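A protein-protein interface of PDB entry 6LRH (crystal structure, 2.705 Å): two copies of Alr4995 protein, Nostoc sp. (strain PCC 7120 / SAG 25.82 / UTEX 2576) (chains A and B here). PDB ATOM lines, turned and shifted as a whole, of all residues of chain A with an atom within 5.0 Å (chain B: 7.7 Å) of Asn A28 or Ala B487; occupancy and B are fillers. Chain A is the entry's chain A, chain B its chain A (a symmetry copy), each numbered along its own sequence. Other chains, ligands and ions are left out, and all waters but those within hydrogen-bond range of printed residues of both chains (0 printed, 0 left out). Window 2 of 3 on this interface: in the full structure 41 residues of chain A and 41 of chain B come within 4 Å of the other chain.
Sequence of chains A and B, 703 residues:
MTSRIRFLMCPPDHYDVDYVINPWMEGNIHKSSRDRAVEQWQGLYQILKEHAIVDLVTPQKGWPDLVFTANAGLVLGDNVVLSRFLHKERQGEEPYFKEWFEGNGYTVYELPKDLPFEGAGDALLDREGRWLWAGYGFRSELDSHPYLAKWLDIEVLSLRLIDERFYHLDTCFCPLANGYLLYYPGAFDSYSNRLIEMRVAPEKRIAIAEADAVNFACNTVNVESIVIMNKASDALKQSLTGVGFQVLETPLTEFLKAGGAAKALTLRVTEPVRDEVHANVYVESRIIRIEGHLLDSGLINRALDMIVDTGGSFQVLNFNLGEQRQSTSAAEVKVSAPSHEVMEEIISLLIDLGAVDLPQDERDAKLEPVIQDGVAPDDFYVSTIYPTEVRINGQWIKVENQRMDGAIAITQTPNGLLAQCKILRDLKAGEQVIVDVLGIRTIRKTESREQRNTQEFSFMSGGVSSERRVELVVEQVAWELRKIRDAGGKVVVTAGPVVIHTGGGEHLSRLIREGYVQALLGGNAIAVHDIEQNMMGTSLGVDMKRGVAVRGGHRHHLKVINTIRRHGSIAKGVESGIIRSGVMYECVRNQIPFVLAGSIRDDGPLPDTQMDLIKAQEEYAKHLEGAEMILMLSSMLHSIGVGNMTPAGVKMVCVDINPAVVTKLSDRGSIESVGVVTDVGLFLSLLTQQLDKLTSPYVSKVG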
ATOM      1  N   VAL A  17     -18.610  22.945 -11.015  1.00  0.00           N
ATOM      2  CA  VAL A  17     -19.278  21.957 -10.203  1.00  0.00           C
ATOM      3  C   VAL A  17     -18.389  20.740 -10.236  1.00  0.00           C
ATOM      4  O   VAL A  17     -18.282  20.097 -11.266  1.00  0.00           O
ATOM      5  CB  VAL A  17     -20.698  21.623 -10.721  1.00  0.00           C
ATOM      6  CG1 VAL A  17     -21.314  20.516  -9.897  1.00  0.00           C
ATOM      7  CG2 VAL A  17     -21.600  22.856 -10.713  1.00  0.00           C
ATOM      8  N   TRP A  24     -29.257  19.389  -6.642  1.00  0.00           N
ATOM      9  CA  TRP A  24     -29.091  20.260  -7.794  1.00  0.00           C
ATOM     10  C   TRP A  24     -27.811  19.962  -8.534  1.00  0.00           C
ATOM     11  O   TRP A  24     -27.734  20.109  -9.737  1.00  0.00           O
ATOM     12  CB  TRP A  24     -29.093  21.723  -7.360  1.00  0.00           C
ATOM     13  CG  TRP A  24     -30.339  22.123  -6.707  1.00  0.00           C
ATOM     14  CD1 TRP A  24     -30.644  21.991  -5.398  1.00  0.00           C
ATOM     15  CD2 TRP A  24     -31.479  22.708  -7.331  1.00  0.00           C
ATOM     16  NE1 TRP A  24     -31.907  22.459  -5.156  1.00  0.00           N
ATOM     17  CE2 TRP A  24     -32.444  22.906  -6.328  1.00  0.00           C
ATOM     18  CE3 TRP A  24     -31.778  23.091  -8.640  1.00  0.00           C
ATOM     19  CZ2 TRP A  24     -33.684  23.466  -6.588  1.00  0.00           C
ATOM     20  CZ3 TRP A  24     -33.009  23.651  -8.897  1.00  0.00           C
ATOM     21  CH2 TRP A  24     -33.947  23.837  -7.875  1.00  0.00           C
ATOM     22  N   MET A  25     -26.796  19.550  -7.793  1.00  0.00           N
ATOM     23  CA  MET A  25     -25.496  19.291  -8.363  1.00  0.00           C
ATOM     24  C   MET A  25     -25.486  18.003  -9.145  1.00  0.00           C
ATOM     25  O   MET A  25     -24.650  17.817 -10.018  1.00  0.00           O
ATOM     26  CB  MET A  25     -24.440  19.257  -7.269  1.00  0.00           C
ATOM     27  CG  MET A  25     -24.372  20.542  -6.486  1.00  0.00           C
ATOM     28  SD  MET A  25     -23.111  20.592  -5.210  1.00  0.00           S
ATOM     29  CE  MET A  25     -21.723  21.123  -6.178  1.00  0.00           C
ATOM     30  N   GLU A  26     -26.426  17.125  -8.828  1.00  0.00           N
ATOM     31  CA  GLU A  26     -26.495  15.802  -9.433  1.00  0.00           C
ATOM     32  C   GLU A  26     -26.683  15.889 -10.938  1.00  0.00           C
ATOM     33  O   GLU A  26     -27.660  16.434 -11.417  1.00  0.00           O
ATOM     34  CB  GLU A  26     -27.626  14.982  -8.795  1.00  0.00           C
ATOM     35  CG  GLU A  26     -27.592  13.480  -9.071  1.00  0.00           C
ATOM     36  CD  GLU A  26     -26.235  12.837  -8.806  1.00  0.00           C
ATOM     37  OE1 GLU A  26     -25.383  12.800  -9.725  1.00  0.00           O
ATOM     38  OE2 GLU A  26     -26.016  12.358  -7.676  1.00  0.00           O
ATOM     39  N   GLY A  27     -25.722  15.361 -11.677  1.00  0.00           N
ATOM     40  CA  GLY A  27     -25.783  15.370 -13.120  1.00  0.00           C
ATOM     41  C   GLY A  27     -25.227  16.635 -13.725  1.00  0.00           C
ATOM     42  O   GLY A  27     -25.299  16.840 -14.926  1.00  0.00           O
ATOM     43  N   ASN A  28     -24.650  17.480 -12.888  1.00  0.00           N
ATOM     44  CA  ASN A  28     -24.246  18.798 -13.311  1.00  0.00           C
ATOM     45  C   ASN A  28     -22.751  18.988 -13.176  1.00  0.00           C
ATOM     46  O   ASN A  28     -22.240  20.077 -13.405  1.00  0.00           O
ATOM     47  CB  ASN A  28     -25.001  19.857 -12.513  1.00  0.00           C
ATOM     48  CG  ASN A  28     -26.202  20.386 -13.250  1.00  0.00           C
ATOM     49  OD1 ASN A  28     -26.240  20.376 -14.472  1.00  0.00           O
ATOM     50  ND2 ASN A  28     -27.195  20.848 -12.513  1.00  0.00           N
ATOM     51  N   ILE A  29     -22.057  17.913 -12.826  1.00  0.00           N
ATOM     52  CA  ILE A  29     -20.609  17.947 -12.660  1.00  0.00           C
ATOM     53  C   ILE A  29     -19.926  18.377 -13.940  1.00  0.00           C
ATOM     54  O   ILE A  29     -20.194  17.836 -15.003  1.00  0.00           O
ATOM     55  CB  ILE A  29     -20.049  16.573 -12.205  1.00  0.00           C
ATOM     56  CG1 ILE A  29     -20.187  16.430 -10.693  1.00  0.00           C
ATOM     57  CG2 ILE A  29     -18.591  16.431 -12.558  1.00  0.00           C
ATOM     58  CD1 ILE A  29     -19.451  15.255 -10.140  1.00  0.00           C
ATOM     59  N   HIS A  30     -19.066  19.381 -13.819  1.00  0.00           N
ATOM     60  CA  HIS A  30     -18.319  19.927 -14.937  1.00  0.00           C
ATOM     61  C   HIS A  30     -19.208  20.380 -16.092  1.00  0.00           C
ATOM     62  O   HIS A  30     -18.801  20.348 -17.238  1.00  0.00           O
ATOM     63  CB  HIS A  30     -17.302  18.903 -15.433  1.00  0.00           C
ATOM     64  CG  HIS A  30     -16.152  18.700 -14.500  1.00  0.00           C
ATOM     65  ND1 HIS A  30     -15.342  19.735 -14.086  1.00  0.00           N
ATOM     66  CD2 HIS A  30     -15.678  17.586 -13.895  1.00  0.00           C
ATOM     67  CE1 HIS A  30     -14.417  19.267 -13.265  1.00  0.00           C
ATOM     68  NE2 HIS A  30     -14.599  17.966 -13.134  1.00  0.00           N
ATOM     69  N   LYS A  31     -20.419  20.809 -15.790  1.00  0.00           N
ATOM     70  CA  LYS A  31     -21.309  21.292 -16.830  1.00  0.00           C
ATOM     71  C   LYS A  31     -21.520  22.787 -16.669  1.00  0.00           C
ATOM     72  O   LYS A  31     -22.321  23.398 -17.366  1.00  0.00           O
ATOM     73  CB  LYS A  31     -22.636  20.535 -16.804  1.00  0.00           C
ATOM     74  CG  LYS A  31     -22.486  19.095 -17.250  1.00  0.00           C
ATOM     75  CD  LYS A  31     -23.796  18.475 -17.682  1.00  0.00           C
ATOM     76  CE  LYS A  31     -23.566  17.467 -18.800  1.00  0.00           C
ATOM     77  NZ  LYS A  31     -24.719  16.552 -19.024  1.00  0.00           N
ATOM     78  N   SER A  32     -20.762  23.361 -15.746  1.00  0.00           N
ATOM     79  CA  SER A  32     -20.735  24.793 -15.533  1.00  0.00           C
ATOM     80  C   SER A  32     -19.915  25.529 -16.581  1.00  0.00           C
ATOM     81  O   SER A  32     -18.794  25.142 -16.887  1.00  0.00           O
ATOM     82  CB  SER A  32     -20.166  25.104 -14.164  1.00  0.00           C
ATOM     83  OG  SER A  32     -19.524  26.368 -14.193  1.00  0.00           O
ATOM     84  N   LYS A 257     -26.988  25.390 -10.942  1.00  0.00           N
ATOM     85  CA  LYS A 257     -26.437  24.075 -11.189  1.00  0.00           C
ATOM     86  C   LYS A 257     -25.683  23.542  -9.970  1.00  0.00           C
ATOM     87  O   LYS A 257     -25.479  22.341  -9.848  1.00  0.00           O
ATOM     88  CB  LYS A 257     -25.527  24.106 -12.404  1.00  0.00           C
ATOM     89  CG  LYS A 257     -26.200  24.555 -13.641  1.00  0.00           C
ATOM     90  CD  LYS A 257     -25.301  24.364 -14.811  1.00  0.00           C
ATOM     91  CE  LYS A 257     -25.679  25.261 -15.964  1.00  0.00           C
ATOM     92  NZ  LYS A 257     -24.583  25.331 -16.950  1.00  0.00           N
ATOM     93  N   LEU B 481     -36.761  15.447 -14.577  1.00  0.00           N
ATOM     94  CA  LEU B 481     -36.776  15.393 -16.025  1.00  0.00           C
ATOM     95  C   LEU B 481     -36.446  16.751 -16.630  1.00  0.00           C
ATOM     96  O   LEU B 481     -35.750  16.835 -17.625  1.00  0.00           O
ATOM     97  CB  LEU B 481     -38.128  14.910 -16.531  1.00  0.00           C
ATOM     98  CG  LEU B 481     -38.448  13.429 -16.389  1.00  0.00           C
ATOM     99  CD1 LEU B 481     -39.894  13.204 -16.807  1.00  0.00           C
ATOM    100  CD2 LEU B 481     -37.500  12.565 -17.209  1.00  0.00           C
ATOM    101  N   ARG B 482     -36.948  17.809 -16.019  1.00  0.00           N
ATOM    102  CA  ARG B 482     -36.692  19.147 -16.503  1.00  0.00           C
ATOM    103  C   ARG B 482     -35.219  19.446 -16.388  1.00  0.00           C
ATOM    104  O   ARG B 482     -34.583  19.861 -17.341  1.00  0.00           O
ATOM    105  CB  ARG B 482     -37.504  20.162 -15.714  1.00  0.00           C
ATOM    106  CG  ARG B 482     -37.398  21.591 -16.199  1.00  0.00           C
ATOM    107  CD  ARG B 482     -37.103  22.490 -14.999  1.00  0.00           C
ATOM    108  NE  ARG B 482     -37.617  23.851 -15.141  1.00  0.00           N
ATOM    109  CZ  ARG B 482     -37.633  24.746 -14.155  1.00  0.00           C
ATOM    110  NH1 ARG B 482     -37.162  24.430 -12.957  1.00  0.00           N
ATOM    111  NH2 ARG B 482     -38.118  25.956 -14.366  1.00  0.00           N
ATOM    112  N   LYS B 483     -34.686  19.223 -15.199  1.00  0.00           N
ATOM    113  CA  LYS B 483     -33.274  19.384 -14.916  1.00  0.00           C
ATOM    114  C   LYS B 483     -32.369  18.690 -15.930  1.00  0.00           C
ATOM    115  O   LYS B 483     -31.471  19.300 -16.498  1.00  0.00           O
ATOM    116  CB  LYS B 483     -33.006  18.842 -13.527  1.00  0.00           C
ATOM    117  CG  LYS B 483     -31.703  19.226 -12.905  1.00  0.00           C
ATOM    118  CD  LYS B 483     -31.692  18.758 -11.466  1.00  0.00           C
ATOM    119  CE  LYS B 483     -30.317  18.842 -10.891  1.00  0.00           C
ATOM    120  NZ  LYS B 483     -29.406  17.837 -11.473  1.00  0.00           N
ATOM    121  N   ILE B 484     -32.618  17.406 -16.154  1.00  0.00           N
ATOM    122  CA  ILE B 484     -31.806  16.621 -17.063  1.00  0.00           C
ATOM    123  C   ILE B 484     -31.935  17.103 -18.501  1.00  0.00           C
ATOM    124  O   ILE B 484     -30.968  17.057 -19.248  1.00  0.00           O
ATOM    125  CB  ILE B 484     -32.159  15.142 -16.990  1.00  0.00           C
ATOM    126  CG1 ILE B 484     -31.958  14.626 -15.576  1.00  0.00           C
ATOM    127  CG2 ILE B 484     -31.268  14.364 -17.892  1.00  0.00           C
ATOM    128  CD1 ILE B 484     -32.525  13.260 -15.320  1.00  0.00           C
ATOM    129  N   ARG B 485     -33.109  17.588 -18.892  1.00  0.00           N
ATOM    130  CA  ARG B 485     -33.276  18.019 -20.268  1.00  0.00           C
ATOM    131  C   ARG B 485     -32.462  19.273 -20.535  1.00  0.00           C
ATOM    132  O   ARG B 485     -31.857  19.395 -21.593  1.00  0.00           O
ATOM    133  CB  ARG B 485     -34.750  18.266 -20.612  1.00  0.00           C
ATOM    134  CG  ARG B 485     -34.982  18.572 -22.096  1.00  0.00           C
ATOM    135  CD  ARG B 485     -36.370  19.127 -22.394  1.00  0.00           C
ATOM    136  NE  ARG B 485     -36.644  20.383 -21.700  1.00  0.00           N
ATOM    137  CZ  ARG B 485     -37.763  21.091 -21.831  1.00  0.00           C
ATOM    138  NH1 ARG B 485     -38.727  20.686 -22.636  1.00  0.00           N
ATOM    139  NH2 ARG B 485     -37.922  22.207 -21.149  1.00  0.00           N
ATOM    140  N   ASP B 486     -32.459  20.199 -19.573  1.00  0.00           N
ATOM    141  CA  ASP B 486     -31.705  21.444 -19.683  1.00  0.00           C
ATOM    142  C   ASP B 486     -30.208  21.209 -19.701  1.00  0.00           C
ATOM    143  O   ASP B 486     -29.467  21.993 -20.258  1.00  0.00           O
ATOM    144  CB  ASP B 486     -32.025  22.386 -18.531  1.00  0.00           C
ATOM    145  CG  ASP B 486     -33.496  22.680 -18.403  1.00  0.00           C
ATOM    146  OD1 ASP B 486     -34.284  22.252 -19.283  1.00  0.00           O
ATOM    147  OD2 ASP B 486     -33.862  23.361 -17.415  1.00  0.00           O
ATOM    148  N   ALA B 487     -29.775  20.125 -19.075  1.00  0.00           N
ATOM    149  CA  ALA B 487     -28.374  19.855 -18.875  1.00  0.00           C
ATOM    150  C   ALA B 487     -27.738  19.108 -20.029  1.00  0.00           C
ATOM    151  O   ALA B 487     -26.529  18.902 -20.046  1.00  0.00           O
ATOM    152  CB  ALA B 487     -28.200  19.088 -17.626  1.00  0.00           C
ATOM    153  N   GLY B 488     -28.554  18.694 -20.989  1.00  0.00           N
ATOM    154  CA  GLY B 488     -28.098  17.836 -22.064  1.00  0.00           C
ATOM    155  C   GLY B 488     -27.833  16.428 -21.587  1.00  0.00           C
ATOM    156  O   GLY B 488     -27.004  15.711 -22.138  1.00  0.00           O
ATOM    157  N   GLY B 489     -28.545  16.028 -20.548  1.00  0.00           N
ATOM    158  CA  GLY B 489     -28.431  14.686 -20.025  1.00  0.00           C
ATOM    159  C   GLY B 489     -29.109  13.651 -20.887  1.00  0.00           C
ATOM    160  O   GLY B 489     -29.461  13.920 -22.020  1.00  0.00           O
ATOM    161  N   LYS B 490     -29.285  12.456 -20.342  1.00  0.00           N
ATOM    162  CA  LYS B 490     -29.841  11.336 -21.085  1.00  0.00           C
ATOM    163  C   LYS B 490     -30.854  10.596 -20.232  1.00  0.00           C
ATOM    164  O   LYS B 490     -30.519  10.058 -19.189  1.00  0.00           O
ATOM    165  CB  LYS B 490     -28.725  10.393 -21.533  1.00  0.00           C
ATOM    166  CG  LYS B 490     -29.197   9.081 -22.125  1.00  0.00           C
ATOM    167  CD  LYS B 490     -28.039   8.186 -22.518  1.00  0.00           C
ATOM    168  CE  LYS B 490     -28.492   7.161 -23.532  1.00  0.00           C
ATOM    169  NZ  LYS B 490     -27.373   6.412 -24.140  1.00  0.00           N
ATOM    170  N   GLU B 628     -28.607   8.855 -17.032  1.00  0.00           N
ATOM    171  CA  GLU B 628     -28.730   9.444 -15.715  1.00  0.00           C
ATOM    172  C   GLU B 628     -30.005   8.983 -15.042  1.00  0.00           C
ATOM    173  O   GLU B 628     -30.061   8.818 -13.835  1.00  0.00           O
ATOM    174  CB  GLU B 628     -28.685  10.964 -15.808  1.00  0.00           C
ATOM    175  CG  GLU B 628     -27.271  11.493 -15.913  1.00  0.00           C
ATOM    176  CD  GLU B 628     -27.139  12.632 -16.884  1.00  0.00           C
ATOM    177  OE1 GLU B 628     -28.083  12.818 -17.666  1.00  0.00           O
ATOM    178  OE2 GLU B 628     -26.100  13.335 -16.874  1.00  0.00           O
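Among the printed residues, no Asp or Glu carboxylate lies within 4 Å of a Lys or Arg side-chain nitrogen of the other chain.
No position is printed for both chains.
O of Trp A24 sits at hydrogen-bond distance from ND2 of Asn A28, at 2.9 Å. The backbone carbonyl oxygen of Lys A31 sits at hydrogen-bond distance from the side-chain amino group of Lys A257, at 3.0 Å.
The backbone carbonyl oxygen (O) of Trp A24 sits close to the side-chain amino group (NZ) of Lys B483 (3.3 Å). The backbone carbonyl oxygen (O) of Ala B487 lies within hydrogen-bond range of the side-chain amino group (NZ) of Lys A31, at 3.1 Å. The backbone carbonyl oxygen of Glu A26 sits close to the side-chain amino group of Lys B483 (2.2 Å).
Among the printed residues, merely in contact across the chains: Asn A28 with Lys B483 (3.9 Å), Asn A28 with Ala B487 (3.9 Å) and Lys A31 with Gly B488 (3.95 Å).
No residue of chain B comes within 4 Å of Gly A27. Asn A28 touches just these residues of chain B: Lys B483 (3.9 Å) and Ala B487 (3.9 Å). Arg B482 touches none of the printed residues of chain A. Printed residues of chain A within 4 Å of Lys B483: Trp A24 (3.1 Å), Glu A26 (2.2 Å) and Asn A28 (3.9 Å). Of the printed residues of chain A, Gly B488 touches Lys A31. The nearest residue of chain B that does not touch Asn A28 is Glu B628 (5.9 Å). The nearest residue of chain A that does not touch Ala B487 is Gly A27 (4.6 Å). The nearest printed residue of chain B that does not touch Glu A26 is Ile B484 (6.2 Å).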
